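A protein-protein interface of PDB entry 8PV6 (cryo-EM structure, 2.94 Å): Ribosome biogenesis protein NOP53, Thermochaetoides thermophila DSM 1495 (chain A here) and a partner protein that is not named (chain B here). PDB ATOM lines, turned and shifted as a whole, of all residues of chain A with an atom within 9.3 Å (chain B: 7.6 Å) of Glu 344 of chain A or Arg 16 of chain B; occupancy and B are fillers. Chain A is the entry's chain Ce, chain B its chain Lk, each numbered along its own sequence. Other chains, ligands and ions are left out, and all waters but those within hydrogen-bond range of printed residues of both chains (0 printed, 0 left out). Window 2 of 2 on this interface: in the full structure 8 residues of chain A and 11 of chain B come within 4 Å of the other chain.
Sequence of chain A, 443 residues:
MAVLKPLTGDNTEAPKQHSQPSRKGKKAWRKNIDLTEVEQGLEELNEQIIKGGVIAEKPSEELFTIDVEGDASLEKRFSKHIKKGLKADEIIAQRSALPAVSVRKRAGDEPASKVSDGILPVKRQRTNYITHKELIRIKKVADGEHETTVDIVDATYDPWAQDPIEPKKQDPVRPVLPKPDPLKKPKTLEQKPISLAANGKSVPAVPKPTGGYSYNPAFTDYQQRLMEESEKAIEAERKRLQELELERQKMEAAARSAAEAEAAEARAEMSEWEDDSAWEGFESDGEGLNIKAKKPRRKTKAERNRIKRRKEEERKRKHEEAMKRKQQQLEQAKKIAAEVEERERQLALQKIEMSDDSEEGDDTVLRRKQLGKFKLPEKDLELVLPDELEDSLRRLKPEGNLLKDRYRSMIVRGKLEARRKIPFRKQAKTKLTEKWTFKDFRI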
ATOM      1  N   LYS A 334      27.176 -27.559  29.932  1.00  0.00           N
ATOM      2  CA  LYS A 334      26.374 -28.787  29.907  1.00  0.00           C
ATOM      3  C   LYS A 334      25.106 -28.663  30.750  1.00  0.00           C
ATOM      4  O   LYS A 334      24.022 -29.103  30.332  1.00  0.00           O
ATOM      5  CB  LYS A 334      27.213 -29.971  30.388  1.00  0.00           C
ATOM      6  CG  LYS A 334      28.345 -30.362  29.453  1.00  0.00           C
ATOM      7  CD  LYS A 334      28.946 -31.698  29.855  1.00  0.00           C
ATOM      8  CE  LYS A 334      30.008 -32.151  28.866  1.00  0.00           C
ATOM      9  NZ  LYS A 334      30.557 -33.489  29.222  1.00  0.00           N
ATOM     10  N   ILE A 336      23.499 -26.049  31.362  1.00  0.00           N
ATOM     11  CA  ILE A 336      22.588 -25.174  30.628  1.00  0.00           C
ATOM     12  C   ILE A 336      21.713 -25.988  29.679  1.00  0.00           C
ATOM     13  O   ILE A 336      20.496 -25.766  29.580  1.00  0.00           O
ATOM     14  CB  ILE A 336      23.391 -24.094  29.881  1.00  0.00           C
ATOM     15  CG1 ILE A 336      24.049 -23.135  30.875  1.00  0.00           C
ATOM     16  CG2 ILE A 336      22.512 -23.338  28.918  1.00  0.00           C
ATOM     17  CD1 ILE A 336      24.947 -22.110  30.226  1.00  0.00           C
ATOM     18  N   ALA A 337      22.319 -26.949  28.974  1.00  0.00           N
ATOM     19  CA  ALA A 337      21.553 -27.849  28.117  1.00  0.00           C
ATOM     20  C   ALA A 337      20.588 -28.698  28.933  1.00  0.00           C
ATOM     21  O   ALA A 337      19.451 -28.945  28.505  1.00  0.00           O
ATOM     22  CB  ALA A 337      22.498 -28.739  27.310  1.00  0.00           C
ATOM     23  N   ALA A 338      21.020 -29.143  30.119  1.00  0.00           N
ATOM     24  CA  ALA A 338      20.118 -29.885  30.997  1.00  0.00           C
ATOM     25  C   ALA A 338      18.916 -29.036  31.411  1.00  0.00           C
ATOM     26  O   ALA A 338      17.773 -29.511  31.383  1.00  0.00           O
ATOM     27  CB  ALA A 338      20.873 -30.382  32.230  1.00  0.00           C
ATOM     28  N   GLU A 339      19.157 -27.769  31.766  1.00  0.00           N
ATOM     29  CA  GLU A 339      18.071 -26.883  32.183  1.00  0.00           C
ATOM     30  C   GLU A 339      17.110 -26.584  31.042  1.00  0.00           C
ATOM     31  O   GLU A 339      15.892 -26.535  31.252  1.00  0.00           O
ATOM     32  CB  GLU A 339      18.622 -25.576  32.754  1.00  0.00           C
ATOM     33  CG  GLU A 339      19.391 -25.726  34.049  1.00  0.00           C
ATOM     34  CD  GLU A 339      20.402 -24.617  34.249  1.00  0.00           C
ATOM     35  OE1 GLU A 339      20.564 -23.786  33.331  1.00  0.00           O
ATOM     36  OE2 GLU A 339      21.040 -24.583  35.322  1.00  0.00           O
ATOM     37  N   VAL A 340      17.626 -26.363  29.830  1.00  0.00           N
ATOM     38  CA  VAL A 340      16.727 -26.032  28.725  1.00  0.00           C
ATOM     39  C   VAL A 340      15.926 -27.264  28.308  1.00  0.00           C
ATOM     40  O   VAL A 340      14.753 -27.159  27.923  1.00  0.00           O
ATOM     41  CB  VAL A 340      17.493 -25.397  27.545  1.00  0.00           C
ATOM     42  CG1 VAL A 340      18.426 -26.372  26.860  1.00  0.00           C
ATOM     43  CG2 VAL A 340      16.522 -24.786  26.541  1.00  0.00           C
ATOM     44  N   GLU A 341      16.523 -28.457  28.431  1.00  0.00           N
ATOM     45  CA  GLU A 341      15.767 -29.673  28.151  1.00  0.00           C
ATOM     46  C   GLU A 341      14.677 -29.888  29.192  1.00  0.00           C
ATOM     47  O   GLU A 341      13.553 -30.276  28.850  1.00  0.00           O
ATOM     48  CB  GLU A 341      16.704 -30.878  28.089  1.00  0.00           C
ATOM     49  CG  GLU A 341      16.001 -32.182  27.750  1.00  0.00           C
ATOM     50  CD  GLU A 341      16.965 -33.277  27.338  1.00  0.00           C
ATOM     51  OE1 GLU A 341      18.147 -32.966  27.077  1.00  0.00           O
ATOM     52  OE2 GLU A 341      16.537 -34.448  27.261  1.00  0.00           O
ATOM     53  N   GLU A 342      14.983 -29.610  30.464  1.00  0.00           N
ATOM     54  CA  GLU A 342      13.982 -29.720  31.523  1.00  0.00           C
ATOM     55  C   GLU A 342      12.847 -28.723  31.314  1.00  0.00           C
ATOM     56  O   GLU A 342      11.670 -29.054  31.502  1.00  0.00           O
ATOM     57  CB  GLU A 342      14.645 -29.509  32.886  1.00  0.00           C
ATOM     58  CG  GLU A 342      13.680 -29.312  34.054  1.00  0.00           C
ATOM     59  CD  GLU A 342      12.959 -30.585  34.468  1.00  0.00           C
ATOM     60  OE1 GLU A 342      13.429 -31.689  34.120  1.00  0.00           O
ATOM     61  OE2 GLU A 342      11.918 -30.480  35.151  1.00  0.00           O
ATOM     62  N   ARG A 343      13.188 -27.496  30.911  1.00  0.00           N
ATOM     63  CA  ARG A 343      12.177 -26.469  30.667  1.00  0.00           C
ATOM     64  C   ARG A 343      11.279 -26.836  29.491  1.00  0.00           C
ATOM     65  O   ARG A 343      10.053 -26.665  29.559  1.00  0.00           O
ATOM     66  CB  ARG A 343      12.861 -25.122  30.429  1.00  0.00           C
ATOM     67  CG  ARG A 343      11.952 -24.004  29.941  1.00  0.00           C
ATOM     68  CD  ARG A 343      10.889 -23.633  30.959  1.00  0.00           C
ATOM     69  NE  ARG A 343      10.056 -22.546  30.461  1.00  0.00           N
ATOM     70  CZ  ARG A 343       9.021 -22.031  31.110  1.00  0.00           C
ATOM     71  NH1 ARG A 343       8.652 -22.488  32.296  1.00  0.00           N
ATOM     72  NH2 ARG A 343       8.334 -21.038  30.552  1.00  0.00           N
ATOM     73  N   GLU A 344      11.862 -27.347  28.402  1.00  0.00           N
ATOM     74  CA  GLU A 344      11.036 -27.760  27.272  1.00  0.00           C
ATOM     75  C   GLU A 344      10.193 -28.979  27.624  1.00  0.00           C
ATOM     76  O   GLU A 344       9.079 -29.134  27.122  1.00  0.00           O
ATOM     77  CB  GLU A 344      11.888 -28.037  26.039  1.00  0.00           C
ATOM     78  CG  GLU A 344      12.476 -26.801  25.392  1.00  0.00           C
ATOM     79  CD  GLU A 344      13.465 -27.178  24.331  1.00  0.00           C
ATOM     80  OE1 GLU A 344      13.835 -28.367  24.312  1.00  0.00           O
ATOM     81  OE2 GLU A 344      13.864 -26.309  23.527  1.00  0.00           O
ATOM     82  N   ARG A 345      10.707 -29.856  28.492  1.00  0.00           N
ATOM     83  CA  ARG A 345       9.898 -30.980  28.956  1.00  0.00           C
ATOM     84  C   ARG A 345       8.709 -30.499  29.781  1.00  0.00           C
ATOM     85  O   ARG A 345       7.593 -31.014  29.636  1.00  0.00           O
ATOM     86  CB  ARG A 345      10.758 -31.949  29.766  1.00  0.00           C
ATOM     87  CG  ARG A 345      10.016 -33.173  30.287  1.00  0.00           C
ATOM     88  CD  ARG A 345      10.667 -33.705  31.554  1.00  0.00           C
ATOM     89  NE  ARG A 345      10.651 -32.731  32.639  1.00  0.00           N
ATOM     90  CZ  ARG A 345       9.644 -32.578  33.490  1.00  0.00           C
ATOM     91  NH1 ARG A 345       8.547 -33.310  33.399  1.00  0.00           N
ATOM     92  NH2 ARG A 345       9.744 -31.669  34.456  1.00  0.00           N
ATOM     93  N   GLN A 346       8.931 -29.499  30.639  1.00  0.00           N
ATOM     94  CA  GLN A 346       7.836 -28.904  31.400  1.00  0.00           C
ATOM     95  C   GLN A 346       6.799 -28.285  30.473  1.00  0.00           C
ATOM     96  O   GLN A 346       5.591 -28.470  30.662  1.00  0.00           O
ATOM     97  CB  GLN A 346       8.376 -27.853  32.370  1.00  0.00           C
ATOM     98  CG  GLN A 346       9.214 -28.406  33.510  1.00  0.00           C
ATOM     99  CD  GLN A 346      10.045 -27.333  34.190  1.00  0.00           C
ATOM    100  OE1 GLN A 346      10.111 -26.196  33.723  1.00  0.00           O
ATOM    101  NE2 GLN A 346      10.684 -27.691  35.298  1.00  0.00           N
ATOM    102  N   LEU A 347       7.261 -27.564  29.445  1.00  0.00           N
ATOM    103  CA  LEU A 347       6.341 -26.967  28.480  1.00  0.00           C
ATOM    104  C   LEU A 347       5.587 -28.034  27.692  1.00  0.00           C
ATOM    105  O   LEU A 347       4.410 -27.854  27.359  1.00  0.00           O
ATOM    106  CB  LEU A 347       7.103 -26.040  27.533  1.00  0.00           C
ATOM    107  CG  LEU A 347       7.555 -24.697  28.108  1.00  0.00           C
ATOM    108  CD1 LEU A 347       8.308 -23.891  27.063  1.00  0.00           C
ATOM    109  CD2 LEU A 347       6.361 -23.914  28.627  1.00  0.00           C
ATOM    110  N   ALA A 348       6.248 -29.157  27.401  1.00  0.00           N
ATOM    111  CA  ALA A 348       5.602 -30.248  26.679  1.00  0.00           C
ATOM    112  C   ALA A 348       4.487 -30.876  27.507  1.00  0.00           C
ATOM    113  O   ALA A 348       3.394 -31.137  26.994  1.00  0.00           O
ATOM    114  CB  ALA A 348       6.641 -31.300  26.286  1.00  0.00           C
ATOM    115  N   LEU A 349       4.745 -31.121  28.797  1.00  0.00           N
ATOM    116  CA  LEU A 349       3.684 -31.646  29.658  1.00  0.00           C
ATOM    117  C   LEU A 349       2.560 -30.632  29.867  1.00  0.00           C
ATOM    118  O   LEU A 349       1.390 -31.020  29.970  1.00  0.00           O
ATOM    119  CB  LEU A 349       4.241 -32.126  31.001  1.00  0.00           C
ATOM    120  CG  LEU A 349       4.841 -33.540  31.093  1.00  0.00           C
ATOM    121  CD1 LEU A 349       6.171 -33.736  30.388  1.00  0.00           C
ATOM    122  CD2 LEU A 349       4.956 -33.949  32.557  1.00  0.00           C
ATOM    123  N   GLN A 350       2.887 -29.336  29.928  1.00  0.00           N
ATOM    124  CA  GLN A 350       1.837 -28.321  30.029  1.00  0.00           C
ATOM    125  C   GLN A 350       0.972 -28.286  28.773  1.00  0.00           C
ATOM    126  O   GLN A 350      -0.248 -28.095  28.850  1.00  0.00           O
ATOM    127  CB  GLN A 350       2.439 -26.942  30.303  1.00  0.00           C
ATOM    128  CG  GLN A 350       3.080 -26.796  31.670  1.00  0.00           C
ATOM    129  CD  GLN A 350       3.898 -25.528  31.793  1.00  0.00           C
ATOM    130  OE1 GLN A 350       3.853 -24.658  30.923  1.00  0.00           O
ATOM    131  NE2 GLN A 350       4.657 -25.416  32.876  1.00  0.00           N
ATOM    132  N   LYS A 351       1.591 -28.458  27.603  1.00  0.00           N
ATOM    133  CA  LYS A 351       0.825 -28.511  26.362  1.00  0.00           C
ATOM    134  C   LYS A 351      -0.013 -29.784  26.287  1.00  0.00           C
ATOM    135  O   LYS A 351      -1.124 -29.775  25.742  1.00  0.00           O
ATOM    136  CB  LYS A 351       1.767 -28.412  25.162  1.00  0.00           C
ATOM    137  CG  LYS A 351       1.070 -28.319  23.812  1.00  0.00           C
ATOM    138  CD  LYS A 351       0.252 -27.043  23.697  1.00  0.00           C
ATOM    139  CE  LYS A 351      -0.411 -26.932  22.332  1.00  0.00           C
ATOM    140  NZ  LYS A 351      -1.288 -25.732  22.237  1.00  0.00           N
ATOM    141  N   ILE A 352       0.510 -30.889  26.826  1.00  0.00           N
ATOM    142  CA  ILE A 352      -0.222 -32.155  26.808  1.00  0.00           C
ATOM    143  C   ILE A 352      -1.451 -32.077  27.709  1.00  0.00           C
ATOM    144  O   ILE A 352      -2.556 -32.469  27.313  1.00  0.00           O
ATOM    145  CB  ILE A 352       0.712 -33.315  27.208  1.00  0.00           C
ATOM    146  CG1 ILE A 352       1.602 -33.708  26.027  1.00  0.00           C
ATOM    147  CG2 ILE A 352      -0.079 -34.525  27.689  1.00  0.00           C
ATOM    148  CD1 ILE A 352       2.703 -34.680  26.389  1.00  0.00           C
ATOM    149  N   LYS B  10      21.257 -19.105  24.676  1.00  0.00           N
ATOM    150  CA  LYS B  10      20.442 -18.699  23.538  1.00  0.00           C
ATOM    151  C   LYS B  10      20.852 -19.449  22.281  1.00  0.00           C
ATOM    152  O   LYS B  10      20.001 -19.814  21.461  1.00  0.00           O
ATOM    153  CB  LYS B  10      20.571 -17.194  23.321  1.00  0.00           C
ATOM    154  CG  LYS B  10      19.912 -16.351  24.393  1.00  0.00           C
ATOM    155  CD  LYS B  10      20.133 -14.869  24.131  1.00  0.00           C
ATOM    156  CE  LYS B  10      19.379 -14.419  22.887  1.00  0.00           C
ATOM    157  NZ  LYS B  10      17.902 -14.488  23.074  1.00  0.00           N
ATOM    158  N   PHE B  11      22.152 -19.717  22.132  1.00  0.00           N
ATOM    159  CA  PHE B  11      22.622 -20.535  21.021  1.00  0.00           C
ATOM    160  C   PHE B  11      22.061 -21.952  21.096  1.00  0.00           C
ATOM    161  O   PHE B  11      21.775 -22.568  20.066  1.00  0.00           O
ATOM    162  CB  PHE B  11      24.149 -20.550  20.998  1.00  0.00           C
ATOM    163  CG  PHE B  11      24.729 -21.032  19.705  1.00  0.00           C
ATOM    164  CD1 PHE B  11      24.711 -20.219  18.583  1.00  0.00           C
ATOM    165  CD2 PHE B  11      25.314 -22.283  19.612  1.00  0.00           C
ATOM    166  CE1 PHE B  11      25.246 -20.650  17.389  1.00  0.00           C
ATOM    167  CE2 PHE B  11      25.861 -22.717  18.418  1.00  0.00           C
ATOM    168  CZ  PHE B  11      25.818 -21.902  17.304  1.00  0.00           C
ATOM    169  N   ILE B  12      21.877 -22.476  22.309  1.00  0.00           N
ATOM    170  CA  ILE B  12      21.322 -23.820  22.465  1.00  0.00           C
ATOM    171  C   ILE B  12      19.841 -23.853  22.083  1.00  0.00           C
ATOM    172  O   ILE B  12      19.403 -24.766  21.368  1.00  0.00           O
ATOM    173  CB  ILE B  12      21.569 -24.345  23.891  1.00  0.00           C
ATOM    174  CG1 ILE B  12      23.044 -24.684  24.062  1.00  0.00           C
ATOM    175  CG2 ILE B  12      20.759 -25.590  24.162  1.00  0.00           C
ATOM    176  CD1 ILE B  12      23.392 -25.129  25.450  1.00  0.00           C
ATOM    177  N   GLU B  13      19.045 -22.857  22.528  1.00  0.00           N
ATOM    178  CA  GLU B  13      17.655 -22.854  22.045  1.00  0.00           C
ATOM    179  C   GLU B  13      17.592 -22.642  20.537  1.00  0.00           C
ATOM    180  O   GLU B  13      16.751 -23.246  19.864  1.00  0.00           O
ATOM    181  CB  GLU B  13      16.679 -21.838  22.682  1.00  0.00           C
ATOM    182  CG  GLU B  13      16.219 -21.935  24.156  1.00  0.00           C
ATOM    183  CD  GLU B  13      17.126 -21.317  25.178  1.00  0.00           C
ATOM    184  OE1 GLU B  13      18.123 -20.713  24.779  1.00  0.00           O
ATOM    185  OE2 GLU B  13      16.819 -21.414  26.387  1.00  0.00           O
ATOM    186  N   ILE B  14      18.485 -21.814  19.987  1.00  0.00           N
ATOM    187  CA  ILE B  14      18.486 -21.558  18.549  1.00  0.00           C
ATOM    188  C   ILE B  14      18.829 -22.825  17.768  1.00  0.00           C
ATOM    189  O   ILE B  14      18.186 -23.143  16.759  1.00  0.00           O
ATOM    190  CB  ILE B  14      19.440 -20.393  18.226  1.00  0.00           C
ATOM    191  CG1 ILE B  14      18.776 -19.067  18.599  1.00  0.00           C
ATOM    192  CG2 ILE B  14      19.793 -20.377  16.764  1.00  0.00           C
ATOM    193  CD1 ILE B  14      19.641 -17.860  18.380  1.00  0.00           C
ATOM    194  N   CYS B  15      19.828 -23.582  18.230  1.00  0.00           N
ATOM    195  CA  CYS B  15      20.168 -24.839  17.571  1.00  0.00           C
ATOM    196  C   CYS B  15      19.057 -25.869  17.711  1.00  0.00           C
ATOM    197  O   CYS B  15      18.812 -26.643  16.779  1.00  0.00           O
ATOM    198  CB  CYS B  15      21.473 -25.399  18.135  1.00  0.00           C
ATOM    199  SG  CYS B  15      22.956 -24.466  17.721  1.00  0.00           S
ATOM    200  N   ARG B  16      18.362 -25.889  18.845  1.00  0.00           N
ATOM    201  CA  ARG B  16      17.327 -26.898  19.029  1.00  0.00           C
ATOM    202  C   ARG B  16      15.987 -26.478  18.416  1.00  0.00           C
ATOM    203  O   ARG B  16      15.067 -27.299  18.335  1.00  0.00           O
ATOM    204  CB  ARG B  16      17.242 -27.221  20.528  1.00  0.00           C
ATOM    205  CG  ARG B  16      16.324 -28.362  20.935  1.00  0.00           C
ATOM    206  CD  ARG B  16      16.379 -28.570  22.428  1.00  0.00           C
ATOM    207  NE  ARG B  16      17.706 -29.008  22.847  1.00  0.00           N
ATOM    208  CZ  ARG B  16      18.114 -30.271  22.828  1.00  0.00           C
ATOM    209  NH1 ARG B  16      17.317 -31.249  22.436  1.00  0.00           N
ATOM    210  NH2 ARG B  16      19.348 -30.561  23.232  1.00  0.00           N
ATOM    211  N   ARG B  17      15.878 -25.234  17.940  1.00  0.00           N
ATOM    212  CA  ARG B  17      14.713 -24.810  17.167  1.00  0.00           C
ATOM    213  C   ARG B  17      14.540 -25.646  15.904  1.00  0.00           C
ATOM    214  O   ARG B  17      15.504 -26.173  15.343  1.00  0.00           O
ATOM    215  CB  ARG B  17      14.831 -23.331  16.793  1.00  0.00           C
ATOM    216  CG  ARG B  17      14.458 -22.350  17.889  1.00  0.00           C
ATOM    217  CD  ARG B  17      14.908 -20.942  17.532  1.00  0.00           C
ATOM    218  NE  ARG B  17      14.646 -20.602  16.140  1.00  0.00           N
ATOM    219  CZ  ARG B  17      15.020 -19.465  15.569  1.00  0.00           C
ATOM    220  NH1 ARG B  17      15.696 -18.546  16.239  1.00  0.00           N
ATOM    221  NH2 ARG B  17      14.714 -19.248  14.294  1.00  0.00           N
ATOM    222  N   LYS B  18      13.286 -25.759  15.462  1.00  0.00           N
ATOM    223  CA  LYS B  18      12.946 -26.692  14.393  1.00  0.00           C
ATOM    224  C   LYS B  18      13.430 -26.195  13.037  1.00  0.00           C
ATOM    225  O   LYS B  18      13.707 -26.998  12.138  1.00  0.00           O
ATOM    226  CB  LYS B  18      11.437 -26.928  14.373  1.00  0.00           C
ATOM    227  CG  LYS B  18      10.919 -27.701  15.576  1.00  0.00           C
ATOM    228  CD  LYS B  18       9.403 -27.843  15.530  1.00  0.00           C
ATOM    229  CE  LYS B  18       8.970 -28.782  14.410  1.00  0.00           C
ATOM    230  NZ  LYS B  18       9.408 -30.183  14.675  1.00  0.00           N
ATOM    231  N   ASP B  19      13.539 -24.877  12.864  1.00  0.00           N
ATOM    232  CA  ASP B  19      13.985 -24.344  11.583  1.00  0.00           C
ATOM    233  C   ASP B  19      15.480 -24.525  11.351  1.00  0.00           C
ATOM    234  O   ASP B  19      15.941 -24.294  10.228  1.00  0.00           O
ATOM    235  CB  ASP B  19      13.628 -22.861  11.472  1.00  0.00           C
ATOM    236  CG  ASP B  19      14.200 -22.041  12.604  1.00  0.00           C
ATOM    237  OD1 ASP B  19      14.637 -22.637  13.609  1.00  0.00           O
ATOM    238  OD2 ASP B  19      14.229 -20.799  12.485  1.00  0.00           O
ATOM    239  N   ALA B  20      16.240 -24.916  12.373  1.00  0.00           N
ATOM    240  CA  ALA B  20      17.679 -25.106  12.224  1.00  0.00           C
ATOM    241  C   ALA B  20      17.965 -26.292  11.314  1.00  0.00           C
ATOM    242  O   ALA B  20      17.682 -27.441  11.668  1.00  0.00           O
ATOM    243  CB  ALA B  20      18.325 -25.313  13.592  1.00  0.00           C
ATOM    244  N   VAL B  51      25.000 -21.501  12.905  1.00  0.00           N
ATOM    245  CA  VAL B  51      23.815 -22.329  12.716  1.00  0.00           C
ATOM    246  C   VAL B  51      22.856 -21.608  11.776  1.00  0.00           C
ATOM    247  O   VAL B  51      22.675 -20.385  11.868  1.00  0.00           O
ATOM    248  CB  VAL B  51      23.164 -22.702  14.066  1.00  0.00           C
ATOM    249  CG1 VAL B  51      22.633 -21.490  14.797  1.00  0.00           C
ATOM    250  CG2 VAL B  51      22.058 -23.731  13.867  1.00  0.00           C
ATOM    251  N   CYS B  53      19.275 -20.971  10.510  1.00  0.00           N
ATOM    252  CA  CYS B  53      17.847 -20.996  10.755  1.00  0.00           C
ATOM    253  C   CYS B  53      17.125 -20.557   9.479  1.00  0.00           C
ATOM    254  O   CYS B  53      17.766 -20.422   8.421  1.00  0.00           O
ATOM    255  CB  CYS B  53      17.536 -20.132  11.974  1.00  0.00           C
ATOM    256  SG  CYS B  53      17.952 -20.905  13.550  1.00  0.00           S
ATOM    257  N   SER B  74      27.522 -31.064  23.154  1.00  0.00           N
ATOM    258  CA  SER B  74      26.274 -30.676  23.807  1.00  0.00           C
ATOM    259  C   SER B  74      25.219 -30.211  22.808  1.00  0.00           C
ATOM    260  O   SER B  74      24.037 -30.133  23.157  1.00  0.00           O
ATOM    261  CB  SER B  74      26.540 -29.580  24.837  1.00  0.00           C
ATOM    262  OG  SER B  74      25.334 -29.167  25.456  1.00  0.00           O
ATOM    263  N   LEU B  75      25.626 -29.871  21.587  1.00  0.00           N
ATOM    264  CA  LEU B  75      24.661 -29.557  20.542  1.00  0.00           C
ATOM    265  C   LEU B  75      23.832 -30.799  20.202  1.00  0.00           C
ATOM    266  O   LEU B  75      24.298 -31.928  20.382  1.00  0.00           O
ATOM    267  CB  LEU B  75      25.373 -29.037  19.290  1.00  0.00           C
ATOM    268  CG  LEU B  75      26.031 -27.654  19.352  1.00  0.00           C
ATOM    269  CD1 LEU B  75      26.242 -27.096  17.954  1.00  0.00           C
ATOM    270  CD2 LEU B  75      25.210 -26.689  20.193  1.00  0.00           C
ATOM    271  N   PRO B  76      22.587 -30.618  19.749  1.00  0.00           N
ATOM    272  CA  PRO B  76      21.704 -31.770  19.474  1.00  0.00           C
ATOM    273  C   PRO B  76      22.254 -32.665  18.376  1.00  0.00           C
ATOM    274  O   PRO B  76      22.871 -32.183  17.414  1.00  0.00           O
ATOM    275  CB  PRO B  76      20.390 -31.107  19.037  1.00  0.00           C
ATOM    276  CG  PRO B  76      20.404 -29.787  19.702  1.00  0.00           C
ATOM    277  CD  PRO B  76      21.840 -29.347  19.730  1.00  0.00           C
ATOM    278  N   PRO B  77      22.049 -33.982  18.490  1.00  0.00           N
ATOM    279  CA  PRO B  77      22.643 -34.896  17.502  1.00  0.00           C
ATOM    280  C   PRO B  77      21.920 -34.902  16.167  1.00  0.00           C
ATOM    281  O   PRO B  77      22.525 -35.259  15.149  1.00  0.00           O
ATOM    282  CB  PRO B  77      22.558 -36.266  18.197  1.00  0.00           C
ATOM    283  CG  PRO B  77      22.238 -35.966  19.643  1.00  0.00           C
ATOM    284  CD  PRO B  77      21.434 -34.711  19.609  1.00  0.00           C
ATOM    285  N   ASN B  78      20.635 -34.537  16.147  1.00  0.00           N
ATOM    286  CA  ASN B  78      19.878 -34.561  14.898  1.00  0.00           C
ATOM    287  C   ASN B  78      20.367 -33.488  13.934  1.00  0.00           C
ATOM    288  O   ASN B  78      20.342 -33.681  12.713  1.00  0.00           O
ATOM    289  CB  ASN B  78      18.389 -34.386  15.184  1.00  0.00           C
ATOM    290  CG  ASN B  78      17.783 -35.593  15.868  1.00  0.00           C
ATOM    291  OD1 ASN B  78      18.080 -36.734  15.517  1.00  0.00           O
ATOM    292  ND2 ASN B  78      16.928 -35.346  16.854  1.00  0.00           N
ATOM    293  N   LEU B  79      20.809 -32.352  14.462  1.00  0.00           N
ATOM    294  CA  LEU B  79      21.315 -31.277  13.621  1.00  0.00           C
ATOM    295  C   LEU B  79      22.693 -31.637  13.081  1.00  0.00           C
ATOM    296  O   LEU B  79      23.612 -31.932  13.851  1.00  0.00           O
ATOM    297  CB  LEU B  79      21.376 -29.980  14.425  1.00  0.00           C
ATOM    298  CG  LEU B  79      21.941 -28.748  13.722  1.00  0.00           C
ATOM    299  CD1 LEU B  79      21.049 -28.355  12.561  1.00  0.00           C
ATOM    300  CD2 LEU B  79      22.088 -27.601  14.706  1.00  0.00           C
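Among the printed residues, merely in contact across the chains: Glu 344 of chain A with Arg 16 of chain B, Val 340 of chain A with Glu 13 of chain B, Ala 337 of chain A with Ser 74 of chain B and Val 340 of chain A with Ile 12 of chain B.
Glu 344 of chain A touches one residue of chain B.
Arg 16 of chain B touches one residue of chain A.
Of the printed residues of chain A, Glu 13 of chain B touches Val 340.
Of the printed residues of chain B, Ala 337 of chain A touches Ser 74.
Printed residues of chain A within 4 Å of Ile 12 of chain B: Val 340.
Of the printed residues of chain A, Ser 74 of chain B touches Ala 337 (3.4 Å).
Arg 17 of chain B touches none of the printed residues of chain A.
The nearest residue of chain B that does not touch Glu 344 of chain A is Glu 13 of chain B (5.0 Å).
The nearest printed residue of chain A that does not touch Glu 13 of chain B is Glu 344 of chain A (5.0 Å).
Of the 19 printed residues of chain B, 4 touch a printed residue of chain A.
Printed residues of chain B that touch a printed residue of chain A: Ile 12, Glu 13, Arg 16 and Ser 74.
Printed residues of chain A that touch a printed residue of chain B: Ala 337, Val 340 and Glu 344.
Among the printed residues, 4 pairs touch across the chains.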
